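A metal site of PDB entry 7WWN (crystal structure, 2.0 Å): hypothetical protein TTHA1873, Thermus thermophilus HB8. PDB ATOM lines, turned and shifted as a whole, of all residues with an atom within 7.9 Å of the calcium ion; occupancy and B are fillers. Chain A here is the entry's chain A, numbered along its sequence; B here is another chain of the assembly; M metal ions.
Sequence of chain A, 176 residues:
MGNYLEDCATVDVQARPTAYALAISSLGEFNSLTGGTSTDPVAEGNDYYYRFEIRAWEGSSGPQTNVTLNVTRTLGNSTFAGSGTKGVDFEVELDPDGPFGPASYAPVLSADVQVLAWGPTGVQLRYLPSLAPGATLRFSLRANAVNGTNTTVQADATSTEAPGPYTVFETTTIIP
Within 4 Å of the calcium ion: Glu 29, Asp 40, Glu 170, Thr 171, Ile 24 of chain B and Ser 25 of chain B.
The backbone NH (N) of Ser 26 of chain B is in hydrogen-bond range of the side-chain carboxylate (OE1) of Glu 170, at 3.1 Å.
The side-chain carboxylate (OD1) of Asp 40 sits at hydrogen-bond distance from the backbone NH (N) of Thr 173 (2.9 Å).
The side-chain hydroxyl of Thr 171 lies within hydrogen-bond range of the backbone carbonyl oxygen of Thr 167 of chain B (2.5 Å).
O of Ser 25 of chain B lies within hydrogen-bond range of N of Glu 53 of chain B, 2.8 Å away.
The side-chain hydroxyl of Thr 172 lies close to the side-chain carboxylate of Glu 29.
The side-chain carboxylate of Glu 170 lies within hydrogen-bond range of the side-chain hydroxyl of Ser 26 of chain A, at 2.5 Å.
The backbone NH (N) of Thr 39 lies within hydrogen-bond range of the backbone carbonyl oxygen (O) of Glu 29, at 3.2 Å.
O of Asp 40 sits at hydrogen-bond distance from NE of Arg 55 of chain B (2.8 Å).
The calcium ion is bound by O of Thr 171 (2.3 Å).
OE2 of Glu 170 is bound to the calcium ion.
O of Ile 24 of chain B binds the calcium ion (2.4 Å).
OD2 of Asp 40 is bound to the calcium ion (2.4 Å).
The side-chain hydroxyl (OG) of Ser 25 of chain B is bound to the calcium ion (2.5 Å).
The side-chain carboxylate (OE2) of Glu 29 is bound to the calcium ion.
OE1 of Glu 29 is bound to the calcium ion.
The calcium ion has seven donor atoms within binding distance.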
ATOM      1  N   SER A  26     -11.614 -38.483   6.016  1.00  0.00           N
ATOM      2  CA  SER A  26     -12.406 -37.222   6.071  1.00  0.00           C
ATOM      3  C   SER A  26     -12.362 -36.490   4.734  1.00  0.00           C
ATOM      4  O   SER A  26     -11.267 -36.398   4.072  1.00  0.00           O
ATOM      5  CB  SER A  26     -11.946 -36.344   7.195  1.00  0.00           C
ATOM      6  OG  SER A  26     -12.744 -35.169   7.282  1.00  0.00           O
ATOM      7  N   LEU A  27     -13.484 -35.902   4.350  1.00  0.00           N
ATOM      8  CA  LEU A  27     -13.614 -35.095   3.110  1.00  0.00           C
ATOM      9  C   LEU A  27     -13.887 -33.656   3.521  1.00  0.00           C
ATOM     10  O   LEU A  27     -14.071 -32.814   2.641  1.00  0.00           O
ATOM     11  CB  LEU A  27     -14.774 -35.615   2.256  1.00  0.00           C
ATOM     12  CG  LEU A  27     -14.659 -37.067   1.779  1.00  0.00           C
ATOM     13  CD1 LEU A  27     -15.767 -37.391   0.786  1.00  0.00           C
ATOM     14  CD2 LEU A  27     -13.326 -37.312   1.143  1.00  0.00           C
ATOM     15  N   GLY A  28     -13.932 -33.411   4.829  1.00  0.00           N
ATOM     16  CA  GLY A  28     -14.232 -32.083   5.365  1.00  0.00           C
ATOM     17  C   GLY A  28     -15.697 -31.734   5.250  1.00  0.00           C
ATOM     18  O   GLY A  28     -16.539 -32.617   4.949  1.00  0.00           O
ATOM     19  N   GLU A  29     -15.985 -30.455   5.451  1.00  0.00           N
ATOM     20  CA  GLU A  29     -17.362 -29.941   5.599  1.00  0.00           C
ATOM     21  C   GLU A  29     -17.888 -29.394   4.273  1.00  0.00           C
ATOM     22  O   GLU A  29     -17.120 -28.889   3.415  1.00  0.00           O
ATOM     23  CB  GLU A  29     -17.453 -28.875   6.693  1.00  0.00           C
ATOM     24  CG  GLU A  29     -16.957 -29.350   8.049  1.00  0.00           C
ATOM     25  CD  GLU A  29     -15.462 -29.224   8.266  1.00  0.00           C
ATOM     26  OE1 GLU A  29     -14.744 -28.892   7.282  1.00  0.00           O
ATOM     27  OE2 GLU A  29     -15.018 -29.402   9.433  1.00  0.00           O
ATOM     28  N   THR A  39     -17.458 -25.787   2.861  1.00  0.00           N
ATOM     29  CA  THR A  39     -17.528 -24.697   3.862  1.00  0.00           C
ATOM     30  C   THR A  39     -16.496 -24.988   4.940  1.00  0.00           C
ATOM     31  O   THR A  39     -15.684 -25.887   4.760  1.00  0.00           O
ATOM     32  CB  THR A  39     -18.945 -24.536   4.405  1.00  0.00           C
ATOM     33  OG1 THR A  39     -18.985 -23.393   5.272  1.00  0.00           O
ATOM     34  CG2 THR A  39     -19.407 -25.766   5.173  1.00  0.00           C
ATOM     35  N   ASP A  40     -16.597 -24.264   6.055  1.00  0.00           N
ATOM     36  CA  ASP A  40     -15.666 -24.235   7.210  1.00  0.00           C
ATOM     37  C   ASP A  40     -14.714 -23.067   6.963  1.00  0.00           C
ATOM     38  O   ASP A  40     -13.953 -23.059   5.985  1.00  0.00           O
ATOM     39  CB  ASP A  40     -14.923 -25.553   7.454  1.00  0.00           C
ATOM     40  CG  ASP A  40     -14.184 -25.571   8.804  1.00  0.00           C
ATOM     41  OD1 ASP A  40     -14.501 -24.709   9.641  1.00  0.00           O
ATOM     42  OD2 ASP A  40     -13.301 -26.450   9.018  1.00  0.00           O
ATOM     43  N   PRO A  41     -14.721 -22.013   7.797  1.00  0.00           N
ATOM     44  CA  PRO A  41     -15.578 -21.910   8.980  1.00  0.00           C
ATOM     45  C   PRO A  41     -17.085 -21.897   8.693  1.00  0.00           C
ATOM     46  O   PRO A  41     -17.493 -21.805   7.538  1.00  0.00           O
ATOM     47  CB  PRO A  41     -15.149 -20.582   9.628  1.00  0.00           C
ATOM     48  CG  PRO A  41     -13.798 -20.266   9.044  1.00  0.00           C
ATOM     49  CD  PRO A  41     -13.830 -20.846   7.643  1.00  0.00           C
ATOM     50  N   TYR A  48     -24.430 -27.219   8.535  1.00  0.00           N
ATOM     51  CA  TYR A  48     -23.343 -27.729   7.660  1.00  0.00           C
ATOM     52  C   TYR A  48     -23.328 -29.257   7.742  1.00  0.00           C
ATOM     53  O   TYR A  48     -24.049 -29.836   8.565  1.00  0.00           O
ATOM     54  CB  TYR A  48     -21.999 -27.115   8.075  1.00  0.00           C
ATOM     55  CG  TYR A  48     -21.468 -27.585   9.405  1.00  0.00           C
ATOM     56  CD1 TYR A  48     -21.948 -27.064  10.596  1.00  0.00           C
ATOM     57  CD2 TYR A  48     -20.424 -28.505   9.472  1.00  0.00           C
ATOM     58  CE1 TYR A  48     -21.453 -27.485  11.818  1.00  0.00           C
ATOM     59  CE2 TYR A  48     -19.896 -28.903  10.696  1.00  0.00           C
ATOM     60  CZ  TYR A  48     -20.407 -28.396  11.871  1.00  0.00           C
ATOM     61  OH  TYR A  48     -19.896 -28.780  13.072  1.00  0.00           O
ATOM     62  N   TYR A  50     -20.692 -32.826   7.607  1.00  0.00           N
ATOM     63  CA  TYR A  50     -19.441 -33.612   7.527  1.00  0.00           C
ATOM     64  C   TYR A  50     -19.629 -34.678   6.460  1.00  0.00           C
ATOM     65  O   TYR A  50     -20.698 -35.268   6.422  1.00  0.00           O
ATOM     66  CB  TYR A  50     -19.116 -34.273   8.859  1.00  0.00           C
ATOM     67  CG  TYR A  50     -18.764 -33.313   9.963  1.00  0.00           C
ATOM     68  CD1 TYR A  50     -17.500 -32.748  10.026  1.00  0.00           C
ATOM     69  CD2 TYR A  50     -19.683 -32.985  10.950  1.00  0.00           C
ATOM     70  CE1 TYR A  50     -17.154 -31.886  11.055  1.00  0.00           C
ATOM     71  CE2 TYR A  50     -19.364 -32.113  11.966  1.00  0.00           C
ATOM     72  CZ  TYR A  50     -18.091 -31.557  12.025  1.00  0.00           C
ATOM     73  OH  TYR A  50     -17.776 -30.683  13.028  1.00  0.00           O
ATOM     74  N   ASN A 150     -14.170 -24.304  18.556  1.00  0.00           N
ATOM     75  CA  ASN A 150     -14.027 -25.308  17.464  1.00  0.00           C
ATOM     76  C   ASN A 150     -14.793 -26.591  17.836  1.00  0.00           C
ATOM     77  O   ASN A 150     -14.710 -27.051  18.992  1.00  0.00           O
ATOM     78  CB  ASN A 150     -12.580 -25.623  17.125  1.00  0.00           C
ATOM     79  CG  ASN A 150     -12.028 -24.743  16.031  1.00  0.00           C
ATOM     80  OD1 ASN A 150     -11.613 -25.216  14.981  1.00  0.00           O
ATOM     81  ND2 ASN A 150     -12.003 -23.447  16.265  1.00  0.00           N
ATOM     82  N   THR A 151     -15.498 -27.158  16.872  1.00  0.00           N
ATOM     83  CA  THR A 151     -16.094 -28.518  16.991  1.00  0.00           C
ATOM     84  C   THR A 151     -15.117 -29.523  16.367  1.00  0.00           C
ATOM     85  O   THR A 151     -14.607 -29.290  15.235  1.00  0.00           O
ATOM     86  CB  THR A 151     -17.469 -28.614  16.329  1.00  0.00           C
ATOM     87  OG1 THR A 151     -18.372 -27.701  16.967  1.00  0.00           O
ATOM     88  CG2 THR A 151     -18.015 -30.012  16.389  1.00  0.00           C
ATOM     89  N   PHE A 169     -10.084 -37.677  12.804  1.00  0.00           N
ATOM     90  CA  PHE A 169     -10.674 -36.502  13.479  1.00  0.00           C
ATOM     91  C   PHE A 169     -10.745 -35.355  12.480  1.00  0.00           C
ATOM     92  O   PHE A 169      -9.718 -35.002  11.884  1.00  0.00           O
ATOM     93  CB  PHE A 169      -9.819 -36.100  14.677  1.00  0.00           C
ATOM     94  CG  PHE A 169      -9.818 -37.073  15.809  1.00  0.00           C
ATOM     95  CD1 PHE A 169      -8.975 -38.172  15.796  1.00  0.00           C
ATOM     96  CD2 PHE A 169     -10.646 -36.884  16.901  1.00  0.00           C
ATOM     97  CE1 PHE A 169      -8.963 -39.052  16.873  1.00  0.00           C
ATOM     98  CE2 PHE A 169     -10.627 -37.757  17.977  1.00  0.00           C
ATOM     99  CZ  PHE A 169      -9.808 -38.863  17.948  1.00  0.00           C
ATOM    100  N   GLU A 170     -11.924 -34.754  12.341  1.00  0.00           N
ATOM    101  CA  GLU A 170     -12.174 -33.560  11.504  1.00  0.00           C
ATOM    102  C   GLU A 170     -12.619 -32.448  12.439  1.00  0.00           C
ATOM    103  O   GLU A 170     -13.288 -32.728  13.439  1.00  0.00           O
ATOM    104  CB  GLU A 170     -13.224 -33.839  10.433  1.00  0.00           C
ATOM    105  CG  GLU A 170     -13.493 -32.665   9.508  1.00  0.00           C
ATOM    106  CD  GLU A 170     -12.255 -32.197   8.752  1.00  0.00           C
ATOM    107  OE1 GLU A 170     -11.601 -33.051   8.059  1.00  0.00           O
ATOM    108  OE2 GLU A 170     -11.935 -30.982   8.852  1.00  0.00           O
ATOM    109  N   THR A 171     -12.226 -31.227  12.111  1.00  0.00           N
ATOM    110  CA  THR A 171     -12.426 -30.046  12.981  1.00  0.00           C
ATOM    111  C   THR A 171     -13.000 -28.895  12.162  1.00  0.00           C
ATOM    112  O   THR A 171     -12.556 -28.655  11.030  1.00  0.00           O
ATOM    113  CB  THR A 171     -11.162 -29.635  13.731  1.00  0.00           C
ATOM    114  OG1 THR A 171     -10.635 -30.789  14.391  1.00  0.00           O
ATOM    115  CG2 THR A 171     -11.425 -28.544  14.740  1.00  0.00           C
ATOM    116  N   THR A 172     -13.951 -28.213  12.776  1.00  0.00           N
ATOM    117  CA  THR A 172     -14.736 -27.115  12.171  1.00  0.00           C
ATOM    118  C   THR A 172     -14.613 -25.913  13.087  1.00  0.00           C
ATOM    119  O   THR A 172     -14.883 -26.057  14.302  1.00  0.00           O
ATOM    120  CB  THR A 172     -16.216 -27.517  12.045  1.00  0.00           C
ATOM    121  OG1 THR A 172     -16.329 -28.887  11.645  1.00  0.00           O
ATOM    122  CG2 THR A 172     -16.946 -26.621  11.067  1.00  0.00           C
ATOM    123  N   THR A 173     -14.234 -24.758  12.535  1.00  0.00           N
ATOM    124  CA  THR A 173     -14.191 -23.488  13.277  1.00  0.00           C
ATOM    125  C   THR A 173     -15.566 -22.869  13.172  1.00  0.00           C
ATOM    126  O   THR A 173     -16.094 -22.770  12.078  1.00  0.00           O
ATOM    127  CB  THR A 173     -13.075 -22.549  12.813  1.00  0.00           C
ATOM    128  OG1 THR A 173     -13.553 -21.805  11.692  1.00  0.00           O
ATOM    129  CG2 THR A 173     -11.807 -23.279  12.415  1.00  0.00           C
ATOM    130  N   ALA B  23      -9.738 -22.025   9.134  1.00  0.00           N
ATOM    131  CA  ALA B  23     -10.185 -23.416   9.322  1.00  0.00           C
ATOM    132  C   ALA B  23      -9.202 -24.340   8.634  1.00  0.00           C
ATOM    133  O   ALA B  23      -8.482 -23.894   7.706  1.00  0.00           O
ATOM    134  CB  ALA B  23     -11.572 -23.612   8.774  1.00  0.00           C
ATOM    135  N   ILE B  24      -9.208 -25.591   9.069  1.00  0.00           N
ATOM    136  CA  ILE B  24      -8.470 -26.697   8.390  1.00  0.00           C
ATOM    137  C   ILE B  24      -9.436 -27.847   8.090  1.00  0.00           C
ATOM    138  O   ILE B  24     -10.404 -28.045   8.844  1.00  0.00           O
ATOM    139  CB  ILE B  24      -7.294 -27.171   9.249  1.00  0.00           C
ATOM    140  CG1 ILE B  24      -6.397 -28.136   8.461  1.00  0.00           C
ATOM    141  CG2 ILE B  24      -7.768 -27.772  10.547  1.00  0.00           C
ATOM    142  CD1 ILE B  24      -5.064 -28.410   9.111  1.00  0.00           C
ATOM    143  N   SER B  25      -9.176 -28.563   7.010  1.00  0.00           N
ATOM    144  CA  SER B  25      -9.899 -29.804   6.663  1.00  0.00           C
ATOM    145  C   SER B  25      -8.931 -30.827   6.054  1.00  0.00           C
ATOM    146  O   SER B  25      -8.033 -30.432   5.279  1.00  0.00           O
ATOM    147  CB  SER B  25     -11.109 -29.546   5.778  1.00  0.00           C
ATOM    148  OG  SER B  25     -12.025 -28.640   6.382  1.00  0.00           O
ATOM    149  N   SER B  26      -9.161 -32.094   6.338  1.00  0.00           N
ATOM    150  CA  SER B  26      -8.593 -33.232   5.563  1.00  0.00           C
ATOM    151  C   SER B  26      -9.436 -33.528   4.327  1.00  0.00           C
ATOM    152  O   SER B  26     -10.718 -33.518   4.390  1.00  0.00           O
ATOM    153  CB  SER B  26      -8.435 -34.448   6.426  1.00  0.00           C
ATOM    154  OG  SER B  26      -7.837 -35.514   5.699  1.00  0.00           O
ATOM    155  N   GLU B  53      -6.677 -28.711   3.462  1.00  0.00           N
ATOM    156  CA  GLU B  53      -7.044 -27.313   3.124  1.00  0.00           C
ATOM    157  C   GLU B  53      -6.892 -26.440   4.357  1.00  0.00           C
ATOM    158  O   GLU B  53      -7.246 -26.861   5.454  1.00  0.00           O
ATOM    159  CB  GLU B  53      -8.463 -27.233   2.580  1.00  0.00           C
ATOM    160  CG  GLU B  53      -8.552 -27.697   1.149  1.00  0.00           C
ATOM    161  CD  GLU B  53      -9.959 -27.564   0.566  1.00  0.00           C
ATOM    162  OE1 GLU B  53     -10.927 -27.816   1.320  1.00  0.00           O
ATOM    163  OE2 GLU B  53     -10.065 -27.209  -0.623  1.00  0.00           O
ATOM    164  N   ARG B  55      -8.410 -22.645   5.180  1.00  0.00           N
ATOM    165  CA  ARG B  55      -9.503 -21.813   4.664  1.00  0.00           C
ATOM    166  C   ARG B  55      -9.613 -20.540   5.514  1.00  0.00           C
ATOM    167  O   ARG B  55      -9.688 -20.643   6.750  1.00  0.00           O
ATOM    168  CB  ARG B  55     -10.794 -22.633   4.648  1.00  0.00           C
ATOM    169  CG  ARG B  55     -10.607 -24.037   4.097  1.00  0.00           C
ATOM    170  CD  ARG B  55     -11.803 -24.923   4.393  1.00  0.00           C
ATOM    171  NE  ARG B  55     -12.980 -24.399   3.715  1.00  0.00           N
ATOM    172  CZ  ARG B  55     -13.381 -24.769   2.509  1.00  0.00           C
ATOM    173  NH1 ARG B  55     -12.684 -25.674   1.839  1.00  0.00           N
ATOM    174  NH2 ARG B  55     -14.443 -24.213   1.966  1.00  0.00           N
ATOM    175  N   TYR B 166      -5.550 -25.068  14.585  1.00  0.00           N
ATOM    176  CA  TYR B 166      -6.715 -25.851  14.124  1.00  0.00           C
ATOM    177  C   TYR B 166      -6.136 -27.193  13.678  1.00  0.00           C
ATOM    178  O   TYR B 166      -5.148 -27.205  12.912  1.00  0.00           O
ATOM    179  CB  TYR B 166      -7.439 -25.085  13.008  1.00  0.00           C
ATOM    180  CG  TYR B 166      -7.819 -23.663  13.360  1.00  0.00           C
ATOM    181  CD1 TYR B 166      -9.027 -23.374  13.950  1.00  0.00           C
ATOM    182  CD2 TYR B 166      -6.966 -22.597  13.089  1.00  0.00           C
ATOM    183  CE1 TYR B 166      -9.401 -22.071  14.272  1.00  0.00           C
ATOM    184  CE2 TYR B 166      -7.318 -21.290  13.383  1.00  0.00           C
ATOM    185  CZ  TYR B 166      -8.536 -21.031  13.992  1.00  0.00           C
ATOM    186  OH  TYR B 166      -8.917 -19.749  14.298  1.00  0.00           O
ATOM    187  N   THR B 167      -6.707 -28.286  14.180  1.00  0.00           N
ATOM    188  CA  THR B 167      -6.065 -29.612  14.139  1.00  0.00           C
ATOM    189  C   THR B 167      -7.030 -30.658  13.564  1.00  0.00           C
ATOM    190  O   THR B 167      -8.167 -30.773  14.055  1.00  0.00           O
ATOM    191  CB  THR B 167      -5.527 -29.988  15.513  1.00  0.00           C
ATOM    192  OG1 THR B 167      -4.512 -29.050  15.889  1.00  0.00           O
ATOM    193  CG2 THR B 167      -4.930 -31.375  15.527  1.00  0.00           C
ATOM    194  N   VAL B 168      -6.546 -31.442  12.612  1.00  0.00           N
ATOM    195  CA  VAL B 168      -7.224 -32.693  12.183  1.00  0.00           C
ATOM    196  C   VAL B 168      -6.217 -33.839  12.238  1.00  0.00           C
ATOM    197  O   VAL B 168      -5.014 -33.599  12.310  1.00  0.00           O
ATOM    198  CB  VAL B 168      -7.844 -32.572  10.784  1.00  0.00           C
ATOM    199  CG1 VAL B 168      -8.987 -31.581  10.782  1.00  0.00           C
ATOM    200  CG2 VAL B 168      -6.797 -32.250   9.725  1.00  0.00           C
HETATM  201 CA    CA M   1     -12.662 -28.775   8.777  1.00  0.00          CA
